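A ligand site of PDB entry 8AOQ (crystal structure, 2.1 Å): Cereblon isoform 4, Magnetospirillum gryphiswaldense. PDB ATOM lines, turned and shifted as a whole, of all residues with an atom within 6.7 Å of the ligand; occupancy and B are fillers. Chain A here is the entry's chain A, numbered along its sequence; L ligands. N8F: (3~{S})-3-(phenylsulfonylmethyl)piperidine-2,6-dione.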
ATOM      1  N   VAL A  48     -11.387  -6.571   2.558  1.00  0.00           N
ATOM      2  CA  VAL A  48     -11.002  -7.816   1.832  1.00  0.00           C
ATOM      3  C   VAL A  48      -9.793  -7.522   0.943  1.00  0.00           C
ATOM      4  O   VAL A  48      -9.540  -6.346   0.642  1.00  0.00           O
ATOM      5  CB  VAL A  48     -12.189  -8.347   1.005  1.00  0.00           C
ATOM      6  CG1 VAL A  48     -13.319  -8.850   1.899  1.00  0.00           C
ATOM      7  CG2 VAL A  48     -12.706  -7.309   0.029  1.00  0.00           C
ATOM      8  N   PHE A  49      -9.082  -8.576   0.542  1.00  0.00           N
ATOM      9  CA  PHE A  49      -7.985  -8.495  -0.450  1.00  0.00           C
ATOM     10  C   PHE A  49      -8.192  -9.534  -1.552  1.00  0.00           C
ATOM     11  O   PHE A  49      -8.623 -10.673  -1.262  1.00  0.00           O
ATOM     12  CB  PHE A  49      -6.617  -8.524   0.253  1.00  0.00           C
ATOM     13  CG  PHE A  49      -6.071  -9.864   0.687  1.00  0.00           C
ATOM     14  CD1 PHE A  49      -6.370 -10.389   1.925  1.00  0.00           C
ATOM     15  CD2 PHE A  49      -5.163 -10.535  -0.122  1.00  0.00           C
ATOM     16  CE1 PHE A  49      -5.820 -11.598   2.336  1.00  0.00           C
ATOM     17  CE2 PHE A  49      -4.606 -11.732   0.291  1.00  0.00           C
ATOM     18  CZ  PHE A  49      -4.952 -12.276   1.509  1.00  0.00           C
ATOM     19  N   ASN A  50      -7.870  -9.131  -2.779  1.00  0.00           N
ATOM     20  CA  ASN A  50      -7.865 -10.013  -3.978  1.00  0.00           C
ATOM     21  C   ASN A  50      -6.517 -10.728  -4.049  1.00  0.00           C
ATOM     22  O   ASN A  50      -5.613 -10.456  -3.265  1.00  0.00           O
ATOM     23  CB  ASN A  50      -8.258  -9.202  -5.219  1.00  0.00           C
ATOM     24  CG  ASN A  50      -7.194  -8.248  -5.709  1.00  0.00           C
ATOM     25  OD1 ASN A  50      -6.066  -8.226  -5.202  1.00  0.00           O
ATOM     26  ND2 ASN A  50      -7.506  -7.510  -6.755  1.00  0.00           N
ATOM     27  N   PRO A  51      -6.355 -11.721  -4.953  1.00  0.00           N
ATOM     28  CA  PRO A  51      -5.097 -12.455  -5.060  1.00  0.00           C
ATOM     29  C   PRO A  51      -3.877 -11.587  -5.404  1.00  0.00           C
ATOM     30  O   PRO A  51      -2.784 -12.007  -5.138  1.00  0.00           O
ATOM     31  CB  PRO A  51      -5.365 -13.465  -6.184  1.00  0.00           C
ATOM     32  CG  PRO A  51      -6.873 -13.642  -6.175  1.00  0.00           C
ATOM     33  CD  PRO A  51      -7.396 -12.265  -5.846  1.00  0.00           C
ATOM     34  N   ALA A  52      -4.095 -10.407  -5.989  1.00  0.00           N
ATOM     35  CA  ALA A  52      -3.014  -9.452  -6.328  1.00  0.00           C
ATOM     36  C   ALA A  52      -2.645  -8.600  -5.093  1.00  0.00           C
ATOM     37  O   ALA A  52      -1.754  -7.751  -5.229  1.00  0.00           O
ATOM     38  CB  ALA A  52      -3.444  -8.610  -7.501  1.00  0.00           C
ATOM     39  N   MET A  54      -4.405  -6.404  -3.410  1.00  0.00           N
ATOM     40  CA  MET A  54      -5.132  -5.114  -3.329  1.00  0.00           C
ATOM     41  C   MET A  54      -6.193  -5.235  -2.225  1.00  0.00           C
ATOM     42  O   MET A  54      -6.923  -6.238  -2.235  1.00  0.00           O
ATOM     43  CB  MET A  54      -5.818  -4.758  -4.651  1.00  0.00           C
ATOM     44  CG  MET A  54      -4.875  -4.637  -5.816  1.00  0.00           C
ATOM     45  SD  MET A  54      -5.774  -4.413  -7.382  1.00  0.00           S
ATOM     46  CE  MET A  54      -6.373  -2.736  -7.146  1.00  0.00           C
ATOM     47  N   PHE A  56      -9.628  -3.730  -0.490  1.00  0.00           N
ATOM     48  CA  PHE A  56     -10.881  -3.002  -0.789  1.00  0.00           C
ATOM     49  C   PHE A  56     -11.673  -2.936   0.512  1.00  0.00           C
ATOM     50  O   PHE A  56     -11.759  -3.978   1.223  1.00  0.00           O
ATOM     51  CB  PHE A  56     -11.687  -3.714  -1.867  1.00  0.00           C
ATOM     52  CG  PHE A  56     -10.944  -3.940  -3.167  1.00  0.00           C
ATOM     53  CD1 PHE A  56     -10.902  -2.971  -4.148  1.00  0.00           C
ATOM     54  CD2 PHE A  56     -10.262  -5.124  -3.391  1.00  0.00           C
ATOM     55  CE1 PHE A  56     -10.219  -3.189  -5.340  1.00  0.00           C
ATOM     56  CE2 PHE A  56      -9.589  -5.345  -4.583  1.00  0.00           C
ATOM     57  CZ  PHE A  56      -9.578  -4.376  -5.551  1.00  0.00           C
ATOM     58  N   GLU A  76     -14.545 -18.207  -8.161  1.00  0.00           N
ATOM     59  CA  GLU A  76     -13.096 -18.208  -7.815  1.00  0.00           C
ATOM     60  C   GLU A  76     -12.758 -17.032  -6.886  1.00  0.00           C
ATOM     61  O   GLU A  76     -13.049 -15.887  -7.247  1.00  0.00           O
ATOM     62  CB  GLU A  76     -12.252 -18.119  -9.078  1.00  0.00           C
ATOM     63  CG  GLU A  76     -12.326 -19.374  -9.929  1.00  0.00           C
ATOM     64  CD  GLU A  76     -11.360 -19.373 -11.093  1.00  0.00           C
ATOM     65  OE1 GLU A  76     -11.157 -18.286 -11.696  1.00  0.00           O
ATOM     66  OE2 GLU A  76     -10.791 -20.461 -11.386  1.00  0.00           O
ATOM     67  N   PHE A  77     -12.192 -17.314  -5.706  1.00  0.00           N
ATOM     68  CA  PHE A  77     -11.709 -16.317  -4.724  1.00  0.00           C
ATOM     69  C   PHE A  77     -12.863 -15.442  -4.220  1.00  0.00           C
ATOM     70  O   PHE A  77     -12.581 -14.328  -3.772  1.00  0.00           O
ATOM     71  CB  PHE A  77     -10.618 -15.440  -5.339  1.00  0.00           C
ATOM     72  CG  PHE A  77      -9.482 -16.193  -5.975  1.00  0.00           C
ATOM     73  CD1 PHE A  77      -8.654 -16.998  -5.205  1.00  0.00           C
ATOM     74  CD2 PHE A  77      -9.248 -16.127  -7.333  1.00  0.00           C
ATOM     75  CE1 PHE A  77      -7.626 -17.727  -5.779  1.00  0.00           C
ATOM     76  CE2 PHE A  77      -8.213 -16.843  -7.916  1.00  0.00           C
ATOM     77  CZ  PHE A  77      -7.397 -17.643  -7.134  1.00  0.00           C
ATOM     78  N   SER A  78     -14.120 -15.900  -4.262  1.00  0.00           N
ATOM     79  CA  SER A  78     -15.275 -15.133  -3.743  1.00  0.00           C
ATOM     80  C   SER A  78     -15.065 -14.869  -2.254  1.00  0.00           C
ATOM     81  O   SER A  78     -14.794 -15.807  -1.527  1.00  0.00           O
ATOM     82  CB  SER A  78     -16.600 -15.821  -3.964  1.00  0.00           C
ATOM     83  OG  SER A  78     -17.639 -14.989  -3.455  1.00  0.00           O
ATOM     84  N   TRP A  79     -15.245 -13.624  -1.829  1.00  0.00           N
ATOM     85  CA  TRP A  79     -15.153 -13.205  -0.400  1.00  0.00           C
ATOM     86  C   TRP A  79     -16.400 -13.645   0.361  1.00  0.00           C
ATOM     87  O   TRP A  79     -16.388 -13.570   1.587  1.00  0.00           O
ATOM     88  CB  TRP A  79     -14.977 -11.691  -0.322  1.00  0.00           C
ATOM     89  CG  TRP A  79     -13.681 -11.254  -0.925  1.00  0.00           C
ATOM     90  CD1 TRP A  79     -12.446 -11.777  -0.686  1.00  0.00           C
ATOM     91  CD2 TRP A  79     -13.500 -10.181  -1.862  1.00  0.00           C
ATOM     92  NE1 TRP A  79     -11.504 -11.091  -1.407  1.00  0.00           N
ATOM     93  CE2 TRP A  79     -12.123 -10.093  -2.116  1.00  0.00           C
ATOM     94  CE3 TRP A  79     -14.362  -9.265  -2.471  1.00  0.00           C
ATOM     95  CZ2 TRP A  79     -11.590  -9.155  -2.990  1.00  0.00           C
ATOM     96  CZ3 TRP A  79     -13.837  -8.333  -3.325  1.00  0.00           C
ATOM     97  CH2 TRP A  79     -12.461  -8.278  -3.574  1.00  0.00           C
ATOM     98  N   PHE A  80     -17.458 -14.024  -0.344  1.00  0.00           N
ATOM     99  CA  PHE A  80     -18.765 -14.349   0.255  1.00  0.00           C
ATOM    100  C   PHE A  80     -19.139 -15.765  -0.167  1.00  0.00           C
ATOM    101  O   PHE A  80     -19.422 -15.981  -1.360  1.00  0.00           O
ATOM    102  CB  PHE A  80     -19.790 -13.294  -0.128  1.00  0.00           C
ATOM    103  CG  PHE A  80     -19.405 -11.889   0.251  1.00  0.00           C
ATOM    104  CD1 PHE A  80     -19.635 -11.417   1.533  1.00  0.00           C
ATOM    105  CD2 PHE A  80     -18.840 -11.039  -0.679  1.00  0.00           C
ATOM    106  CE1 PHE A  80     -19.308 -10.105   1.874  1.00  0.00           C
ATOM    107  CE2 PHE A  80     -18.497  -9.745  -0.331  1.00  0.00           C
ATOM    108  CZ  PHE A  80     -18.748  -9.277   0.941  1.00  0.00           C
ATOM    109  N   TYR A  83     -21.533 -17.419  -3.162  1.00  0.00           N
ATOM    110  CA  TYR A  83     -21.827 -16.369  -4.164  1.00  0.00           C
ATOM    111  C   TYR A  83     -20.767 -16.355  -5.254  1.00  0.00           C
ATOM    112  O   TYR A  83     -19.580 -16.430  -4.958  1.00  0.00           O
ATOM    113  CB  TYR A  83     -21.921 -14.989  -3.526  1.00  0.00           C
ATOM    114  CG  TYR A  83     -23.075 -14.836  -2.587  1.00  0.00           C
ATOM    115  CD1 TYR A  83     -24.329 -14.508  -3.065  1.00  0.00           C
ATOM    116  CD2 TYR A  83     -22.920 -15.068  -1.234  1.00  0.00           C
ATOM    117  CE1 TYR A  83     -25.405 -14.385  -2.198  1.00  0.00           C
ATOM    118  CE2 TYR A  83     -23.978 -14.933  -0.347  1.00  0.00           C
ATOM    119  CZ  TYR A  83     -25.224 -14.600  -0.845  1.00  0.00           C
ATOM    120  OH  TYR A  83     -26.254 -14.421   0.016  1.00  0.00           O
ATOM    121  N   TRP A  85     -19.288 -13.907  -8.415  1.00  0.00           N
ATOM    122  CA  TRP A  85     -19.172 -12.447  -8.623  1.00  0.00           C
ATOM    123  C   TRP A  85     -19.064 -12.133 -10.107  1.00  0.00           C
ATOM    124  O   TRP A  85     -18.518 -12.952 -10.867  1.00  0.00           O
ATOM    125  CB  TRP A  85     -17.999 -11.871  -7.838  1.00  0.00           C
ATOM    126  CG  TRP A  85     -16.726 -12.602  -8.068  1.00  0.00           C
ATOM    127  CD1 TRP A  85     -16.217 -13.608  -7.300  1.00  0.00           C
ATOM    128  CD2 TRP A  85     -15.790 -12.404  -9.141  1.00  0.00           C
ATOM    129  NE1 TRP A  85     -15.057 -14.057  -7.835  1.00  0.00           N
ATOM    130  CE2 TRP A  85     -14.769 -13.362  -8.976  1.00  0.00           C
ATOM    131  CE3 TRP A  85     -15.735 -11.538 -10.239  1.00  0.00           C
ATOM    132  CZ2 TRP A  85     -13.689 -13.462  -9.850  1.00  0.00           C
ATOM    133  CZ3 TRP A  85     -14.666 -11.633 -11.101  1.00  0.00           C
ATOM    134  CH2 TRP A  85     -13.666 -12.590 -10.914  1.00  0.00           C
ATOM    135  N   THR A  86     -19.542 -10.953 -10.478  1.00  0.00           N
ATOM    136  CA  THR A  86     -19.241 -10.295 -11.758  1.00  0.00           C
ATOM    137  C   THR A  86     -18.720  -8.897 -11.431  1.00  0.00           C
ATOM    138  O   THR A  86     -19.255  -8.282 -10.499  1.00  0.00           O
ATOM    139  CB  THR A  86     -20.467 -10.286 -12.678  1.00  0.00           C
ATOM    140  OG1 THR A  86     -21.470  -9.493 -12.067  1.00  0.00           O
ATOM    141  CG2 THR A  86     -21.028 -11.670 -12.899  1.00  0.00           C
ATOM    142  N   ILE A  87     -17.711  -8.455 -12.152  1.00  0.00           N
ATOM    143  CA  ILE A  87     -17.174  -7.073 -12.021  1.00  0.00           C
ATOM    144  C   ILE A  87     -18.275  -6.081 -12.397  1.00  0.00           C
ATOM    145  O   ILE A  87     -18.947  -6.293 -13.425  1.00  0.00           O
ATOM    146  CB  ILE A  87     -15.916  -6.916 -12.893  1.00  0.00           C
ATOM    147  CG1 ILE A  87     -14.755  -7.711 -12.272  1.00  0.00           C
ATOM    148  CG2 ILE A  87     -15.552  -5.446 -13.070  1.00  0.00           C
ATOM    149  CD1 ILE A  87     -13.677  -8.084 -13.275  1.00  0.00           C
ATOM    150  N   HIS A  96     -14.128   1.081 -12.102  1.00  0.00           N
ATOM    151  CA  HIS A  96     -14.434  -0.171 -11.362  1.00  0.00           C
ATOM    152  C   HIS A  96     -15.015   0.193  -9.996  1.00  0.00           C
ATOM    153  O   HIS A  96     -14.286   0.761  -9.196  1.00  0.00           O
ATOM    154  CB  HIS A  96     -13.196  -1.062 -11.247  1.00  0.00           C
ATOM    155  CG  HIS A  96     -13.486  -2.294 -10.475  1.00  0.00           C
ATOM    156  ND1 HIS A  96     -12.561  -2.876  -9.631  1.00  0.00           N
ATOM    157  CD2 HIS A  96     -14.618  -3.027 -10.363  1.00  0.00           C
ATOM    158  CE1 HIS A  96     -13.080  -3.953  -9.092  1.00  0.00           C
ATOM    159  NE2 HIS A  96     -14.355  -4.063  -9.498  1.00  0.00           N
ATOM    160  N   GLY A  98     -17.078  -2.060  -8.026  1.00  0.00           N
ATOM    161  CA  GLY A  98     -17.145  -3.258  -7.166  1.00  0.00           C
ATOM    162  C   GLY A  98     -17.633  -4.469  -7.935  1.00  0.00           C
ATOM    163  O   GLY A  98     -17.134  -4.720  -9.036  1.00  0.00           O
ATOM    164  N   TRP A  99     -18.551  -5.222  -7.348  1.00  0.00           N
ATOM    165  CA  TRP A  99     -18.973  -6.554  -7.846  1.00  0.00           C
ATOM    166  C   TRP A  99     -20.452  -6.763  -7.600  1.00  0.00           C
ATOM    167  O   TRP A  99     -20.981  -6.265  -6.584  1.00  0.00           O
ATOM    168  CB  TRP A  99     -18.138  -7.658  -7.159  1.00  0.00           C
ATOM    169  CG  TRP A  99     -16.677  -7.492  -7.369  1.00  0.00           C
ATOM    170  CD1 TRP A  99     -15.922  -7.980  -8.392  1.00  0.00           C
ATOM    171  CD2 TRP A  99     -15.787  -6.715  -6.552  1.00  0.00           C
ATOM    172  NE1 TRP A  99     -14.622  -7.590  -8.252  1.00  0.00           N
ATOM    173  CE2 TRP A  99     -14.509  -6.809  -7.138  1.00  0.00           C
ATOM    174  CE3 TRP A  99     -15.944  -5.964  -5.379  1.00  0.00           C
ATOM    175  CZ2 TRP A  99     -13.393  -6.178  -6.594  1.00  0.00           C
ATOM    176  CZ3 TRP A  99     -14.853  -5.316  -4.851  1.00  0.00           C
ATOM    177  CH2 TRP A  99     -13.591  -5.432  -5.458  1.00  0.00           C
ATOM    178  N   TYR A 101     -22.921  -9.948  -6.813  1.00  0.00           N
ATOM    179  CA  TYR A 101     -22.881 -11.318  -6.260  1.00  0.00           C
ATOM    180  C   TYR A 101     -24.222 -11.998  -6.559  1.00  0.00           C
ATOM    181  O   TYR A 101     -25.257 -11.352  -6.443  1.00  0.00           O
ATOM    182  CB  TYR A 101     -22.563 -11.255  -4.778  1.00  0.00           C
ATOM    183  CG  TYR A 101     -21.123 -10.866  -4.528  1.00  0.00           C
ATOM    184  CD1 TYR A 101     -20.122 -11.815  -4.513  1.00  0.00           C
ATOM    185  CD2 TYR A 101     -20.772  -9.549  -4.310  1.00  0.00           C
ATOM    186  CE1 TYR A 101     -18.793 -11.475  -4.271  1.00  0.00           C
ATOM    187  CE2 TYR A 101     -19.468  -9.188  -4.043  1.00  0.00           C
ATOM    188  CZ  TYR A 101     -18.466 -10.146  -4.039  1.00  0.00           C
ATOM    189  OH  TYR A 101     -17.160  -9.804  -3.846  1.00  0.00           O
HETATM  190  N1  N8F L   1     -13.169 -11.832  -4.738  1.00  0.00           N
HETATM  191  C4  N8F L   1     -14.455 -11.376  -4.901  1.00  0.00           C
HETATM  192  C5  N8F L   1     -14.710 -10.450  -6.046  1.00  0.00           C
HETATM  193  C6  N8F L   1     -11.258 -10.618  -7.724  1.00  0.00           C
HETATM  194  C7  N8F L   1     -10.034  -9.785 -10.089  1.00  0.00           C
HETATM  195  C8  N8F L   1     -10.688 -10.090 -11.284  1.00  0.00           C
HETATM  196  C10 N8F L   1      -8.593 -10.754 -12.231  1.00  0.00           C
HETATM  197  C1  N8F L   1     -13.674 -10.578  -7.143  1.00  0.00           C
HETATM  198  C2  N8F L   1     -12.263 -10.447  -6.583  1.00  0.00           C
HETATM  199  C3  N8F L   1     -12.048 -11.415  -5.441  1.00  0.00           C
HETATM  200  O1  N8F L   1     -10.956 -11.822  -5.123  1.00  0.00           O
HETATM  201  O2  N8F L   1     -15.326 -11.709  -4.115  1.00  0.00           O
HETATM  202  S1  N8F L   1     -10.955  -9.167  -8.719  1.00  0.00           S
HETATM  203  C9  N8F L   1      -9.955 -10.578 -12.346  1.00  0.00           C
HETATM  204  C11 N8F L   1      -7.944 -10.436 -11.054  1.00  0.00           C
HETATM  205  C12 N8F L   1      -8.662  -9.958  -9.974  1.00  0.00           C
HETATM  206  O3  N8F L   1     -12.185  -8.591  -9.204  1.00  0.00           O
HETATM  207  O4  N8F L   1     -10.093  -8.329  -7.933  1.00  0.00           O
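O2 of the ligand lies within hydrogen-bond range of N of Trp 79, at 3.0 Å.
OH of Tyr 101 lies within hydrogen-bond range of O2 of the ligand.
The backbone carbonyl oxygen (O) of Phe 77 lies within hydrogen-bond range of a nitrogen (N1) of the ligand (2.7 Å).
The side-chain amide nitrogen (ND2) of Asn 50 is in hydrogen-bond range of an oxygen (O4) of the ligand, at 3.0 Å.
An oxygen (O3) of the ligand lies within hydrogen-bond range of the indole nitrogen (NE1) of Trp 99 (2.8 Å).
The side-chain hydroxyl of Ser 78 is in hydrogen-bond range of the backbone carbonyl oxygen of Tyr 83, at 2.8 Å.
O of Phe 80 is in hydrogen-bond range of OG of Ser 78, at 2.9 Å.
The indole nitrogen (NE1) of Trp 79 is in hydrogen-bond range of the backbone carbonyl oxygen (O) of Phe 49 (2.9 Å).
N of Ala 52 is in hydrogen-bond range of OD1 of Asn 50, 3.0 Å away.
OD1 of Asn 50 lies within hydrogen-bond range of N of Met 54.
NE1 of Trp 85 is in hydrogen-bond range of O of Glu 76 (2.8 Å).
Residues that only touch the ligand: Trp 85 (3.4 Å), Ser 78 (3.4 Å) and Pro 51 (3.7 Å).
Hydrophobic or aromatic side chains that line the ligand: Pro 51, Phe 77, Trp 79, Trp 85, Trp 99 and Tyr 101.
Within 4 Å of the ligand: Asn 50, Pro 51, Phe 77, Ser 78, Trp 79, Trp 85, Trp 99 and Tyr 101.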
